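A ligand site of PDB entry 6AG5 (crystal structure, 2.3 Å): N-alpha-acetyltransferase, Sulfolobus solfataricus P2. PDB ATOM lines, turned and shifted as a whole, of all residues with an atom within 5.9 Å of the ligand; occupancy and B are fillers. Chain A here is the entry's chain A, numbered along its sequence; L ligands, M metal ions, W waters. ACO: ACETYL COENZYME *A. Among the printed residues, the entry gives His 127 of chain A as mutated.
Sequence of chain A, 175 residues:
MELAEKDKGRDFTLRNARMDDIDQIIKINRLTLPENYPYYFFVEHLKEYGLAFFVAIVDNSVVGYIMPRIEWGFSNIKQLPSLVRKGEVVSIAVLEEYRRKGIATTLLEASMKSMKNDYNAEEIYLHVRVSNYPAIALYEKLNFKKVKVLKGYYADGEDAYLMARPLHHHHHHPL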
ATOM      1  N   THR A  32      28.913   5.736 -11.082  1.00  0.00           N
ATOM      2  CA  THR A  32      27.661   6.061 -10.373  1.00  0.00           C
ATOM      3  C   THR A  32      26.650   6.903 -11.137  1.00  0.00           C
ATOM      4  O   THR A  32      25.518   7.062 -10.686  1.00  0.00           O
ATOM      5  CB  THR A  32      27.955   6.817  -9.076  1.00  0.00           C
ATOM      6  OG1 THR A  32      28.588   8.072  -9.384  1.00  0.00           O
ATOM      7  CG2 THR A  32      28.857   5.993  -8.163  1.00  0.00           C
ATOM      8  N   LEU A  33      27.066   7.465 -12.269  1.00  0.00           N
ATOM      9  CA  LEU A  33      26.208   8.391 -13.013  1.00  0.00           C
ATOM     10  C   LEU A  33      26.287   8.129 -14.510  1.00  0.00           C
ATOM     11  O   LEU A  33      27.344   7.762 -15.024  1.00  0.00           O
ATOM     12  CB  LEU A  33      26.596   9.846 -12.746  1.00  0.00           C
ATOM     13  CG  LEU A  33      26.277  10.418 -11.377  1.00  0.00           C
ATOM     14  CD1 LEU A  33      27.102  11.677 -11.096  1.00  0.00           C
ATOM     15  CD2 LEU A  33      24.789  10.681 -11.304  1.00  0.00           C
ATOM     16  N   TYR A  37      30.956  13.463 -17.896  1.00  0.00           N
ATOM     17  CA  TYR A  37      31.706  14.613 -18.373  1.00  0.00           C
ATOM     18  C   TYR A  37      33.127  14.234 -18.759  1.00  0.00           C
ATOM     19  O   TYR A  37      33.745  13.399 -18.094  1.00  0.00           O
ATOM     20  CB  TYR A  37      31.719  15.708 -17.293  1.00  0.00           C
ATOM     21  CG  TYR A  37      30.358  15.989 -16.677  1.00  0.00           C
ATOM     22  CD1 TYR A  37      29.391  16.722 -17.362  1.00  0.00           C
ATOM     23  CD2 TYR A  37      30.055  15.543 -15.392  1.00  0.00           C
ATOM     24  CE1 TYR A  37      28.148  16.991 -16.772  1.00  0.00           C
ATOM     25  CE2 TYR A  37      28.821  15.802 -14.799  1.00  0.00           C
ATOM     26  CZ  TYR A  37      27.868  16.516 -15.490  1.00  0.00           C
ATOM     27  OH  TYR A  37      26.644  16.755 -14.894  1.00  0.00           O
ATOM     28  N   VAL A  89      25.497  23.092  -8.215  1.00  0.00           N
ATOM     29  CA  VAL A  89      26.050  21.761  -8.046  1.00  0.00           C
ATOM     30  C   VAL A  89      25.919  21.014  -9.364  1.00  0.00           C
ATOM     31  O   VAL A  89      24.854  20.477  -9.689  1.00  0.00           O
ATOM     32  CB  VAL A  89      25.340  20.960  -6.957  1.00  0.00           C
ATOM     33  CG1 VAL A  89      26.050  19.625  -6.780  1.00  0.00           C
ATOM     34  CG2 VAL A  89      25.350  21.724  -5.648  1.00  0.00           C
ATOM     35  N   VAL A  90      27.016  20.970 -10.110  1.00  0.00           N
ATOM     36  CA  VAL A  90      27.002  20.361 -11.444  1.00  0.00           C
ATOM     37  C   VAL A  90      26.925  18.843 -11.354  1.00  0.00           C
ATOM     38  O   VAL A  90      26.295  18.175 -12.181  1.00  0.00           O
ATOM     39  CB  VAL A  90      28.253  20.772 -12.231  1.00  0.00           C
ATOM     40  CG1 VAL A  90      28.339  20.038 -13.585  1.00  0.00           C
ATOM     41  CG2 VAL A  90      28.298  22.296 -12.386  1.00  0.00           C
ATOM     42  N   SER A  91      27.579  18.298 -10.334  1.00  0.00           N
ATOM     43  CA  SER A  91      27.657  16.863 -10.129  1.00  0.00           C
ATOM     44  C   SER A  91      28.126  16.563  -8.713  1.00  0.00           C
ATOM     45  O   SER A  91      28.997  17.255  -8.163  1.00  0.00           O
ATOM     46  CB  SER A  91      28.611  16.232 -11.139  1.00  0.00           C
ATOM     47  OG  SER A  91      28.552  14.824 -11.114  1.00  0.00           O
ATOM     48  N   ILE A  92      27.544  15.527  -8.121  1.00  0.00           N
ATOM     49  CA  ILE A  92      27.996  15.052  -6.845  1.00  0.00           C
ATOM     50  C   ILE A  92      27.761  13.557  -6.820  1.00  0.00           C
ATOM     51  O   ILE A  92      26.759  13.076  -7.333  1.00  0.00           O
ATOM     52  CB  ILE A  92      27.254  15.763  -5.677  1.00  0.00           C
ATOM     53  CG1 ILE A  92      27.695  15.198  -4.329  1.00  0.00           C
ATOM     54  CG2 ILE A  92      25.731  15.642  -5.845  1.00  0.00           C
ATOM     55  CD1 ILE A  92      26.934  15.839  -3.171  1.00  0.00           C
ATOM     56  N   ALA A  93      28.705  12.808  -6.256  1.00  0.00           N
ATOM     57  CA  ALA A  93      28.496  11.379  -6.112  1.00  0.00           C
ATOM     58  C   ALA A  93      29.427  10.812  -5.074  1.00  0.00           C
ATOM     59  O   ALA A  93      30.542  11.307  -4.878  1.00  0.00           O
ATOM     60  CB  ALA A  93      28.691  10.665  -7.434  1.00  0.00           C
ATOM     61  N   VAL A  94      28.925   9.779  -4.400  1.00  0.00           N
ATOM     62  CA  VAL A  94      29.675   9.058  -3.396  1.00  0.00           C
ATOM     63  C   VAL A  94      29.686   7.598  -3.817  1.00  0.00           C
ATOM     64  O   VAL A  94      28.686   7.121  -4.352  1.00  0.00           O
ATOM     65  CB  VAL A  94      29.040   9.240  -2.001  1.00  0.00           C
ATOM     66  CG1 VAL A  94      29.777   8.413  -0.962  1.00  0.00           C
ATOM     67  CG2 VAL A  94      28.998  10.732  -1.605  1.00  0.00           C
ATOM     68  N   LEU A  95      30.782   6.871  -3.616  1.00  0.00           N
ATOM     69  CA  LEU A  95      30.754   5.456  -4.007  1.00  0.00           C
ATOM     70  C   LEU A  95      29.792   4.661  -3.121  1.00  0.00           C
ATOM     71  O   LEU A  95      29.556   4.998  -1.949  1.00  0.00           O
ATOM     72  CB  LEU A  95      32.156   4.840  -3.950  1.00  0.00           C
ATOM     73  CG  LEU A  95      33.159   5.333  -4.984  1.00  0.00           C
ATOM     74  CD1 LEU A  95      34.537   4.813  -4.659  1.00  0.00           C
ATOM     75  CD2 LEU A  95      32.731   4.885  -6.372  1.00  0.00           C
ATOM     76  N   TYR A  98      30.487   3.692   0.553  1.00  0.00           N
ATOM     77  CA  TYR A  98      30.636   4.697   1.593  1.00  0.00           C
ATOM     78  C   TYR A  98      29.373   5.530   1.789  1.00  0.00           C
ATOM     79  O   TYR A  98      29.391   6.566   2.455  1.00  0.00           O
ATOM     80  CB  TYR A  98      31.847   5.585   1.262  1.00  0.00           C
ATOM     81  CG  TYR A  98      33.091   4.780   1.001  1.00  0.00           C
ATOM     82  CD1 TYR A  98      33.917   4.379   2.050  1.00  0.00           C
ATOM     83  CD2 TYR A  98      33.439   4.401  -0.287  1.00  0.00           C
ATOM     84  CE1 TYR A  98      35.068   3.628   1.814  1.00  0.00           C
ATOM     85  CE2 TYR A  98      34.578   3.642  -0.544  1.00  0.00           C
ATOM     86  CZ  TYR A  98      35.390   3.260   0.512  1.00  0.00           C
ATOM     87  OH  TYR A  98      36.520   2.501   0.250  1.00  0.00           O
ATOM     88  N   ARG A  99      28.257   5.060   1.235  1.00  0.00           N
ATOM     89  CA  ARG A  99      26.988   5.758   1.372  1.00  0.00           C
ATOM     90  C   ARG A  99      26.398   5.639   2.772  1.00  0.00           C
ATOM     91  O   ARG A  99      26.781   4.758   3.563  1.00  0.00           O
ATOM     92  CB  ARG A  99      25.976   5.242   0.335  1.00  0.00           C
ATOM     93  CG  ARG A  99      26.252   5.839  -1.036  1.00  0.00           C
ATOM     94  CD  ARG A  99      25.521   5.135  -2.171  1.00  0.00           C
ATOM     95  NE  ARG A  99      26.061   5.600  -3.444  1.00  0.00           N
ATOM     96  CZ  ARG A  99      25.820   5.042  -4.622  1.00  0.00           C
ATOM     97  NH1 ARG A  99      25.023   3.973  -4.720  1.00  0.00           N
ATOM     98  NH2 ARG A  99      26.374   5.545  -5.718  1.00  0.00           N
ATOM     99  N   ARG A 100      25.471   6.563   3.071  1.00  0.00           N
ATOM    100  CA  ARG A 100      24.761   6.626   4.348  1.00  0.00           C
ATOM    101  C   ARG A 100      25.668   6.936   5.538  1.00  0.00           C
ATOM    102  O   ARG A 100      25.359   6.572   6.656  1.00  0.00           O
ATOM    103  CB  ARG A 100      23.991   5.326   4.652  1.00  0.00           C
ATOM    104  CG  ARG A 100      23.024   4.877   3.580  1.00  0.00           C
ATOM    105  CD  ARG A 100      22.128   5.986   3.052  1.00  0.00           C
ATOM    106  NE  ARG A 100      21.129   6.513   3.996  1.00  0.00           N
ATOM    107  CZ  ARG A 100      19.918   6.007   4.186  1.00  0.00           C
ATOM    108  NH1 ARG A 100      19.555   4.914   3.533  1.00  0.00           N
ATOM    109  NH2 ARG A 100      19.071   6.593   5.029  1.00  0.00           N
ATOM    110  N   LYS A 101      26.777   7.627   5.293  1.00  0.00           N
ATOM    111  CA  LYS A 101      27.704   7.953   6.369  1.00  0.00           C
ATOM    112  C   LYS A 101      27.799   9.455   6.567  1.00  0.00           C
ATOM    113  O   LYS A 101      28.631   9.935   7.354  1.00  0.00           O
ATOM    114  CB  LYS A 101      29.091   7.351   6.070  1.00  0.00           C
ATOM    115  CG  LYS A 101      29.076   5.822   6.032  1.00  0.00           C
ATOM    116  CD  LYS A 101      30.432   5.259   5.650  1.00  0.00           C
ATOM    117  CE  LYS A 101      30.448   3.733   5.758  1.00  0.00           C
ATOM    118  NZ  LYS A 101      30.889   3.298   7.115  1.00  0.00           N
ATOM    119  N   GLY A 102      26.955  10.187   5.848  1.00  0.00           N
ATOM    120  CA  GLY A 102      26.991  11.649   5.866  1.00  0.00           C
ATOM    121  C   GLY A 102      27.957  12.268   4.863  1.00  0.00           C
ATOM    122  O   GLY A 102      28.212  13.463   4.909  1.00  0.00           O
ATOM    123  N   ILE A 103      28.498  11.478   3.940  1.00  0.00           N
ATOM    124  CA  ILE A 103      29.553  12.015   3.058  1.00  0.00           C
ATOM    125  C   ILE A 103      28.982  13.060   2.102  1.00  0.00           C
ATOM    126  O   ILE A 103      29.472  14.192   2.077  1.00  0.00           O
ATOM    127  CB  ILE A 103      30.272  10.895   2.248  1.00  0.00           C
ATOM    128  CG1 ILE A 103      31.082   9.993   3.178  1.00  0.00           C
ATOM    129  CG2 ILE A 103      31.205  11.485   1.221  1.00  0.00           C
ATOM    130  CD1 ILE A 103      32.100   9.136   2.463  1.00  0.00           C
ATOM    131  N   ALA A 104      27.952  12.700   1.346  1.00  0.00           N
ATOM    132  CA  ALA A 104      27.281  13.662   0.459  1.00  0.00           C
ATOM    133  C   ALA A 104      26.821  14.921   1.208  1.00  0.00           C
ATOM    134  O   ALA A 104      26.968  16.038   0.713  1.00  0.00           O
ATOM    135  CB  ALA A 104      26.104  13.016  -0.239  1.00  0.00           C
ATOM    136  N   THR A 105      26.260  14.739   2.394  1.00  0.00           N
ATOM    137  CA  THR A 105      25.868  15.873   3.198  1.00  0.00           C
ATOM    138  C   THR A 105      27.019  16.827   3.437  1.00  0.00           C
ATOM    139  O   THR A 105      26.914  18.010   3.144  1.00  0.00           O
ATOM    140  CB  THR A 105      25.296  15.428   4.548  1.00  0.00           C
ATOM    141  OG1 THR A 105      24.079  14.712   4.318  1.00  0.00           O
ATOM    142  CG2 THR A 105      24.997  16.638   5.417  1.00  0.00           C
ATOM    143  N   THR A 106      28.130  16.294   3.943  1.00  0.00           N
ATOM    144  CA  THR A 106      29.252  17.146   4.348  1.00  0.00           C
ATOM    145  C   THR A 106      29.894  17.809   3.129  1.00  0.00           C
ATOM    146  O   THR A 106      30.255  18.986   3.188  1.00  0.00           O
ATOM    147  CB  THR A 106      30.301  16.356   5.189  1.00  0.00           C
ATOM    148  OG1 THR A 106      30.842  15.286   4.410  1.00  0.00           O
ATOM    149  CG2 THR A 106      29.666  15.752   6.420  1.00  0.00           C
ATOM    150  N   LEU A 126      20.454  23.115  -8.736  1.00  0.00           N
ATOM    151  CA  LEU A 126      20.930  21.855  -9.312  1.00  0.00           C
ATOM    152  C   LEU A 126      19.807  21.223 -10.104  1.00  0.00           C
ATOM    153  O   LEU A 126      18.655  21.663 -10.042  1.00  0.00           O
ATOM    154  CB  LEU A 126      21.432  20.882  -8.233  1.00  0.00           C
ATOM    155  CG  LEU A 126      20.527  20.514  -7.041  1.00  0.00           C
ATOM    156  CD1 LEU A 126      19.395  19.582  -7.452  1.00  0.00           C
ATOM    157  CD2 LEU A 126      21.361  19.837  -5.959  1.00  0.00           C
ATOM    158  N   HIS A 127      20.147  20.169 -10.833  1.00  0.00           N
ATOM    159  CA  HIS A 127      19.145  19.367 -11.523  1.00  0.00           C
ATOM    160  C   HIS A 127      19.251  17.962 -10.983  1.00  0.00           C
ATOM    161  O   HIS A 127      20.360  17.486 -10.690  1.00  0.00           O
ATOM    162  CB  HIS A 127      19.370  19.345 -13.039  1.00  0.00           C
ATOM    163  CG  HIS A 127      19.331  20.697 -13.699  1.00  0.00           C
ATOM    164  ND1 HIS A 127      18.182  21.233 -14.239  1.00  0.00           N
ATOM    165  CD2 HIS A 127      20.315  21.601 -13.914  1.00  0.00           C
ATOM    166  CE1 HIS A 127      18.463  22.410 -14.763  1.00  0.00           C
ATOM    167  NE2 HIS A 127      19.739  22.660 -14.580  1.00  0.00           N
ATOM    168  N   VAL A 128      18.123  17.267 -10.866  1.00  0.00           N
ATOM    169  CA  VAL A 128      18.133  15.849 -10.501  1.00  0.00           C
ATOM    170  C   VAL A 128      17.011  15.090 -11.241  1.00  0.00           C
ATOM    171  O   VAL A 128      15.944  15.670 -11.541  1.00  0.00           O
ATOM    172  CB  VAL A 128      17.990  15.682  -8.977  1.00  0.00           C
ATOM    173  CG1 VAL A 128      16.676  16.329  -8.524  1.00  0.00           C
ATOM    174  CG2 VAL A 128      18.048  14.222  -8.578  1.00  0.00           C
ATOM    175  N   ARG A 129      17.248  13.819 -11.562  1.00  0.00           N
ATOM    176  CA  ARG A 129      16.220  12.988 -12.189  1.00  0.00           C
ATOM    177  C   ARG A 129      15.009  12.885 -11.274  1.00  0.00           C
ATOM    178  O   ARG A 129      15.161  12.779 -10.060  1.00  0.00           O
ATOM    179  CB  ARG A 129      16.751  11.597 -12.507  1.00  0.00           C
ATOM    180  CG  ARG A 129      18.017  11.590 -13.324  1.00  0.00           C
ATOM    181  CD  ARG A 129      18.517  10.166 -13.550  1.00  0.00           C
ATOM    182  NE  ARG A 129      19.450  10.102 -14.673  1.00  0.00           N
ATOM    183  CZ  ARG A 129      19.118   9.752 -15.921  1.00  0.00           C
ATOM    184  NH1 ARG A 129      17.865   9.394 -16.211  1.00  0.00           N
ATOM    185  NH2 ARG A 129      20.033   9.756 -16.870  1.00  0.00           N
ATOM    186  N   ASN A 132      15.225  10.071  -8.876  1.00  0.00           N
ATOM    187  CA  ASN A 132      16.403   9.860  -8.026  1.00  0.00           C
ATOM    188  C   ASN A 132      16.037  10.210  -6.589  1.00  0.00           C
ATOM    189  O   ASN A 132      16.513  11.208  -6.036  1.00  0.00           O
ATOM    190  CB  ASN A 132      17.589  10.684  -8.498  1.00  0.00           C
ATOM    191  CG  ASN A 132      18.908  10.209  -7.908  1.00  0.00           C
ATOM    192  OD1 ASN A 132      18.923   9.379  -6.997  1.00  0.00           O
ATOM    193  ND2 ASN A 132      20.030  10.743  -8.425  1.00  0.00           N
ATOM    194  N   TYR A 133      15.154   9.397  -6.022  1.00  0.00           N
ATOM    195  CA  TYR A 133      14.624   9.631  -4.686  1.00  0.00           C
ATOM    196  C   TYR A 133      15.670   9.785  -3.567  1.00  0.00           C
ATOM    197  O   TYR A 133      15.489  10.635  -2.683  1.00  0.00           O
ATOM    198  CB  TYR A 133      13.634   8.518  -4.331  1.00  0.00           C
ATOM    199  CG  TYR A 133      12.442   8.594  -5.244  1.00  0.00           C
ATOM    200  CD1 TYR A 133      11.564   9.668  -5.162  1.00  0.00           C
ATOM    201  CD2 TYR A 133      12.216   7.617  -6.208  1.00  0.00           C
ATOM    202  CE1 TYR A 133      10.474   9.771  -6.011  1.00  0.00           C
ATOM    203  CE2 TYR A 133      11.123   7.712  -7.073  1.00  0.00           C
ATOM    204  CZ  TYR A 133      10.256   8.781  -6.950  1.00  0.00           C
ATOM    205  OH  TYR A 133       9.170   8.902  -7.784  1.00  0.00           O
ATOM    206  N   PRO A 134      16.742   8.984  -3.589  1.00  0.00           N
ATOM    207  CA  PRO A 134      17.707   9.219  -2.505  1.00  0.00           C
ATOM    208  C   PRO A 134      18.360  10.592  -2.621  1.00  0.00           C
ATOM    209  O   PRO A 134      18.635  11.243  -1.618  1.00  0.00           O
ATOM    210  CB  PRO A 134      18.745   8.114  -2.685  1.00  0.00           C
ATOM    211  CG  PRO A 134      18.077   7.058  -3.568  1.00  0.00           C
ATOM    212  CD  PRO A 134      17.133   7.824  -4.433  1.00  0.00           C
ATOM    213  N   ALA A 135      18.619  11.039  -3.849  1.00  0.00           N
ATOM    214  CA  ALA A 135      19.289  12.320  -4.039  1.00  0.00           C
ATOM    215  C   ALA A 135      18.348  13.516  -3.742  1.00  0.00           C
ATOM    216  O   ALA A 135      18.736  14.465  -3.060  1.00  0.00           O
ATOM    217  CB  ALA A 135      19.859  12.402  -5.468  1.00  0.00           C
ATOM    218  N   ALA A 137      15.859  13.385  -1.650  1.00  0.00           N
ATOM    219  CA  ALA A 137      15.724  13.377  -0.191  1.00  0.00           C
ATOM    220  C   ALA A 137      16.881  14.116   0.486  1.00  0.00           C
ATOM    221  O   ALA A 137      16.684  14.884   1.453  1.00  0.00           O
ATOM    222  CB  ALA A 137      15.629  11.966   0.336  1.00  0.00           C
ATOM    223  N   LEU A 138      18.086  13.875  -0.017  1.00  0.00           N
ATOM    224  CA  LEU A 138      19.283  14.500   0.526  1.00  0.00           C
ATOM    225  C   LEU A 138      19.247  16.019   0.311  1.00  0.00           C
ATOM    226  O   LEU A 138      19.615  16.789   1.199  1.00  0.00           O
ATOM    227  CB  LEU A 138      20.526  13.906  -0.124  1.00  0.00           C
ATOM    228  CG  LEU A 138      21.779  14.769  -0.166  1.00  0.00           C
ATOM    229  CD1 LEU A 138      22.515  14.770   1.182  1.00  0.00           C
ATOM    230  CD2 LEU A 138      22.680  14.344  -1.315  1.00  0.00           C
ATOM    231  N   TYR A 139      18.809  16.442  -0.870  1.00  0.00           N
ATOM    232  CA  TYR A 139      18.688  17.858  -1.184  1.00  0.00           C
ATOM    233  C   TYR A 139      17.634  18.531  -0.296  1.00  0.00           C
ATOM    234  O   TYR A 139      17.889  19.596   0.302  1.00  0.00           O
ATOM    235  CB  TYR A 139      18.357  18.051  -2.664  1.00  0.00           C
ATOM    236  CG  TYR A 139      19.428  17.472  -3.575  1.00  0.00           C
ATOM    237  CD1 TYR A 139      20.737  17.328  -3.129  1.00  0.00           C
ATOM    238  CD2 TYR A 139      19.125  17.039  -4.876  1.00  0.00           C
ATOM    239  CE1 TYR A 139      21.715  16.783  -3.936  1.00  0.00           C
ATOM    240  CE2 TYR A 139      20.113  16.496  -5.701  1.00  0.00           C
ATOM    241  CZ  TYR A 139      21.400  16.376  -5.217  1.00  0.00           C
ATOM    242  OH  TYR A 139      22.393  15.848  -5.990  1.00  0.00           O
ATOM    243  N   LYS A 141      16.575  17.691   2.601  1.00  0.00           N
ATOM    244  CA  LYS A 141      17.129  17.776   3.949  1.00  0.00           C
ATOM    245  C   LYS A 141      17.976  19.033   4.092  1.00  0.00           C
ATOM    246  O   LYS A 141      18.110  19.598   5.174  1.00  0.00           O
ATOM    247  CB  LYS A 141      17.979  16.539   4.269  1.00  0.00           C
ATOM    248  CG  LYS A 141      17.265  15.439   5.008  1.00  0.00           C
ATOM    249  CD  LYS A 141      18.275  14.439   5.585  1.00  0.00           C
ATOM    250  CE  LYS A 141      17.597  13.466   6.527  1.00  0.00           C
ATOM    251  NZ  LYS A 141      16.408  12.877   5.854  1.00  0.00           N
ATOM    252  N   TYR A 154      17.135  14.658 -19.405  1.00  0.00           N
ATOM    253  CA  TYR A 154      18.270  13.738 -19.502  1.00  0.00           C
ATOM    254  C   TYR A 154      18.324  12.990 -20.841  1.00  0.00           C
ATOM    255  O   TYR A 154      17.304  12.834 -21.525  1.00  0.00           O
ATOM    256  CB  TYR A 154      18.236  12.760 -18.315  1.00  0.00           C
ATOM    257  CG  TYR A 154      18.508  13.464 -17.003  1.00  0.00           C
ATOM    258  CD1 TYR A 154      19.810  13.641 -16.548  1.00  0.00           C
ATOM    259  CD2 TYR A 154      17.472  13.984 -16.256  1.00  0.00           C
ATOM    260  CE1 TYR A 154      20.069  14.288 -15.357  1.00  0.00           C
ATOM    261  CE2 TYR A 154      17.716  14.660 -15.058  1.00  0.00           C
ATOM    262  CZ  TYR A 154      19.024  14.809 -14.615  1.00  0.00           C
ATOM    263  OH  TYR A 154      19.283  15.466 -13.423  1.00  0.00           O
HETATM  264  N1A ACO L   1      17.660   6.127   0.656  1.00  0.00           N
HETATM  265  C2A ACO L   1      16.865   6.972   1.381  1.00  0.00           C
HETATM  266  N3A ACO L   1      17.346   8.168   1.815  1.00  0.00           N
HETATM  267  C4A ACO L   1      18.652   8.528   1.531  1.00  0.00           C
HETATM  268  C5A ACO L   1      19.428   7.691   0.819  1.00  0.00           C
HETATM  269  C6A ACO L   1      18.926   6.465   0.380  1.00  0.00           C
HETATM  270  N6A ACO L   1      19.427   5.417  -0.349  1.00  0.00           N
HETATM  271  N7A ACO L   1      20.646   8.282   0.681  1.00  0.00           N
HETATM  272  C8A ACO L   1      20.599   9.482   1.310  1.00  0.00           C
HETATM  273  N9A ACO L   1      19.368   9.649   1.833  1.00  0.00           N
HETATM  274  C1B ACO L   1      18.970  10.799   2.590  1.00  0.00           C
HETATM  275  C2B ACO L   1      18.714  10.438   3.856  1.00  0.00           C
HETATM  276  O2B ACO L   1      17.630  11.238   4.442  1.00  0.00           O
HETATM  277  C3B ACO L   1      20.016  10.717   4.618  1.00  0.00           C
HETATM  278  O3B ACO L   1      19.828  10.894   5.958  1.00  0.00           O
HETATM  279  P3B ACO L   1      20.099   9.632   6.941  1.00  0.00           P
HETATM  280  O7A ACO L   1      20.458  10.125   8.271  1.00  0.00           O
HETATM  281  O8A ACO L   1      18.829   8.779   7.056  1.00  0.00           O
HETATM  282  O9A ACO L   1      21.214   8.741   6.359  1.00  0.00           O
HETATM  283  C4B ACO L   1      20.562  11.999   3.902  1.00  0.00           C
HETATM  284  O4B ACO L   1      20.196  11.860   2.643  1.00  0.00           O
HETATM  285  C5B ACO L   1      22.063  12.055   4.023  1.00  0.00           C
HETATM  286  O5B ACO L   1      22.646  11.153   3.120  1.00  0.00           O
HETATM  287  P1A ACO L   1      24.208  11.016   3.026  1.00  0.00           P
HETATM  288  O1A ACO L   1      24.690   9.770   3.784  1.00  0.00           O
HETATM  289  O2A ACO L   1      24.854  12.264   3.657  1.00  0.00           O
HETATM  290  O3A ACO L   1      24.516  10.892   1.461  1.00  0.00           O
HETATM  291  P2A ACO L   1      25.412   9.723   0.781  1.00  0.00           P
HETATM  292  O4A ACO L   1      26.816   9.936   1.301  1.00  0.00           O
HETATM  293  O5A ACO L   1      24.886   8.363   1.159  1.00  0.00           O
HETATM  294  O6A ACO L   1      25.326   9.833  -0.849  1.00  0.00           O
HETATM  295  CBP ACO L   1      24.185  10.168  -3.000  1.00  0.00           C
HETATM  296  CCP ACO L   1      24.147  10.372  -1.418  1.00  0.00           C
HETATM  297  CDP ACO L   1      25.063  11.293  -3.722  1.00  0.00           C
HETATM  298  CEP ACO L   1      22.735  10.234  -3.505  1.00  0.00           C
HETATM  299  CAP ACO L   1      24.730   8.801  -3.261  1.00  0.00           C
HETATM  300  OAP ACO L   1      23.690   7.890  -2.927  1.00  0.00           O
HETATM  301  C9P ACO L   1      25.182   8.599  -4.719  1.00  0.00           C
HETATM  302  O9P ACO L   1      26.351   8.817  -5.034  1.00  0.00           O
HETATM  303  N8P ACO L   1      24.259   8.176  -5.667  1.00  0.00           N
HETATM  304  C7P ACO L   1      24.643   7.992  -7.045  1.00  0.00           C
HETATM  305  C6P ACO L   1      25.090   9.382  -7.686  1.00  0.00           C
HETATM  306  C5P ACO L   1      23.985  10.440  -7.633  1.00  0.00           C
HETATM  307  O5P ACO L   1      22.782  10.120  -7.644  1.00  0.00           O
HETATM  308  N4P ACO L   1      24.340  11.851  -7.590  1.00  0.00           N
HETATM  309  C3P ACO L   1      23.300  12.873  -7.551  1.00  0.00           C
HETATM  310  C2P ACO L   1      22.719  13.089  -8.975  1.00  0.00           C
HETATM  311  S1P ACO L   1      21.978  14.697  -9.083  1.00  0.00           S
HETATM  312  C   ACO L   1      23.221  15.910  -9.511  1.00  0.00           C
HETATM  313  O   ACO L   1      24.157  15.645 -10.231  1.00  0.00           O
HETATM  314  CH3 ACO L   1      23.350  17.148  -8.645  1.00  0.00           C
HETATM  315 CA    CA M   1      19.780  12.391 -11.028  1.00  0.00          CA
HETATM  316  O   HOH W   1      28.073   8.684   3.160  1.00  0.00           O
HETATM  317  O   HOH W   2      23.081   7.265  -0.319  1.00  0.00           O
HETATM  318  O   HOH W   3      23.594   9.564   6.440  1.00  0.00           O
HETATM  319  O   HOH W   4      15.346   9.847   3.540  1.00  0.00           O
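N of Arg 100 sits at hydrogen-bond distance from O5A of the ligand.
O1A of the ligand lies within hydrogen-bond range of N of Lys 101, at 3.4 Å.
NH2 of Arg 100 is in salt-bridge range of O8A of the ligand.
The guanidinium group (NE) of Arg 99 lies within hydrogen-bond range of an oxygen (OAP) of the ligand.
N of Val 94 sits at hydrogen-bond distance from O9P of the ligand (2.8 Å).
NZ of Lys 141 lies within hydrogen-bond range of O2B of the ligand, at 2.5 Å.
A sulfur (S1P) of the ligand sits close to the side-chain hydroxyl of Tyr 139.
O2A of the ligand is in hydrogen-bond range of N of Thr 105, at 3.1 Å.
A nitrogen (N4P) of the ligand is in hydrogen-bond range of the backbone carbonyl oxygen (O) of Ile 92, at 2.7 Å.
An oxygen (O4A) of the ligand is in hydrogen-bond range of the backbone NH (N) of Ile 103, 3.5 Å away.
The side-chain hydroxyl (OG1) of Thr 105 lies within hydrogen-bond range of an oxygen (O2A) of the ligand (2.7 Å).
O1A of the ligand is in hydrogen-bond range of N of Gly 102 (3.1 Å).
The side-chain amide nitrogen of Asn 132 is in hydrogen-bond range of an oxygen (O5P) of the ligand.
An oxygen (O4A) of the ligand lies within hydrogen-bond range of the backbone NH of Ala 104 (3.0 Å).
OH of Tyr 37 sits at hydrogen-bond distance from O of Val 90 (3.1 Å).
O of Gly 102 sits close to OG1 of Thr 106 (3.2 Å).
The guanidinium group of Arg 99 sits at hydrogen-bond distance from the backbone carbonyl oxygen of Val 94 (3.1 Å).
The side-chain hydroxyl (OH) of Tyr 154 lies close to the backbone NH (N) of Val 128, 3.3 Å away.
The side-chain hydroxyl of Thr 106 sits at hydrogen-bond distance from the backbone carbonyl oxygen of Ile 103 (2.9 Å).
O of His 127 sits close to S1P of the ligand.
Residues that only touch the ligand: Leu 138 (3.5 Å), Pro 134 (3.5 Å), Ala 93 (3.5 Å), Ser 91 (3.7 Å), Leu 33 (3.8 Å), Val 89 (3.8 Å), Thr 32 (3.8 Å), Val 90 (3.8 Å) and Val 128 (3.99 Å).
Hydrophobic or aromatic side chains that line the ligand: Leu 33, Ile 92, Ala 93, Val 94, Ile 103, Ala 104, Val 128, Pro 134 and Leu 138.
22 residues have an atom within 4 Å of the ligand: Thr 32, Leu 33, Val 89, Val 90, Ser 91, Ile 92, Ala 93, Val 94, Arg 99, Arg 100, Lys 101, Gly 102, Ile 103, Ala 104, Thr 105, His 127, Val 128, Asn 132, Pro 134, Leu 138, Tyr 139 and Lys 141.
The nearest printed residue that does not touch the ligand is Ala 135 (4.05 Å).
Water W3 lies within hydrogen-bond range of an oxygen (O9A) of the ligand, the backbone NH of Gly 102 and the backbone carbonyl oxygen of Arg 100.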
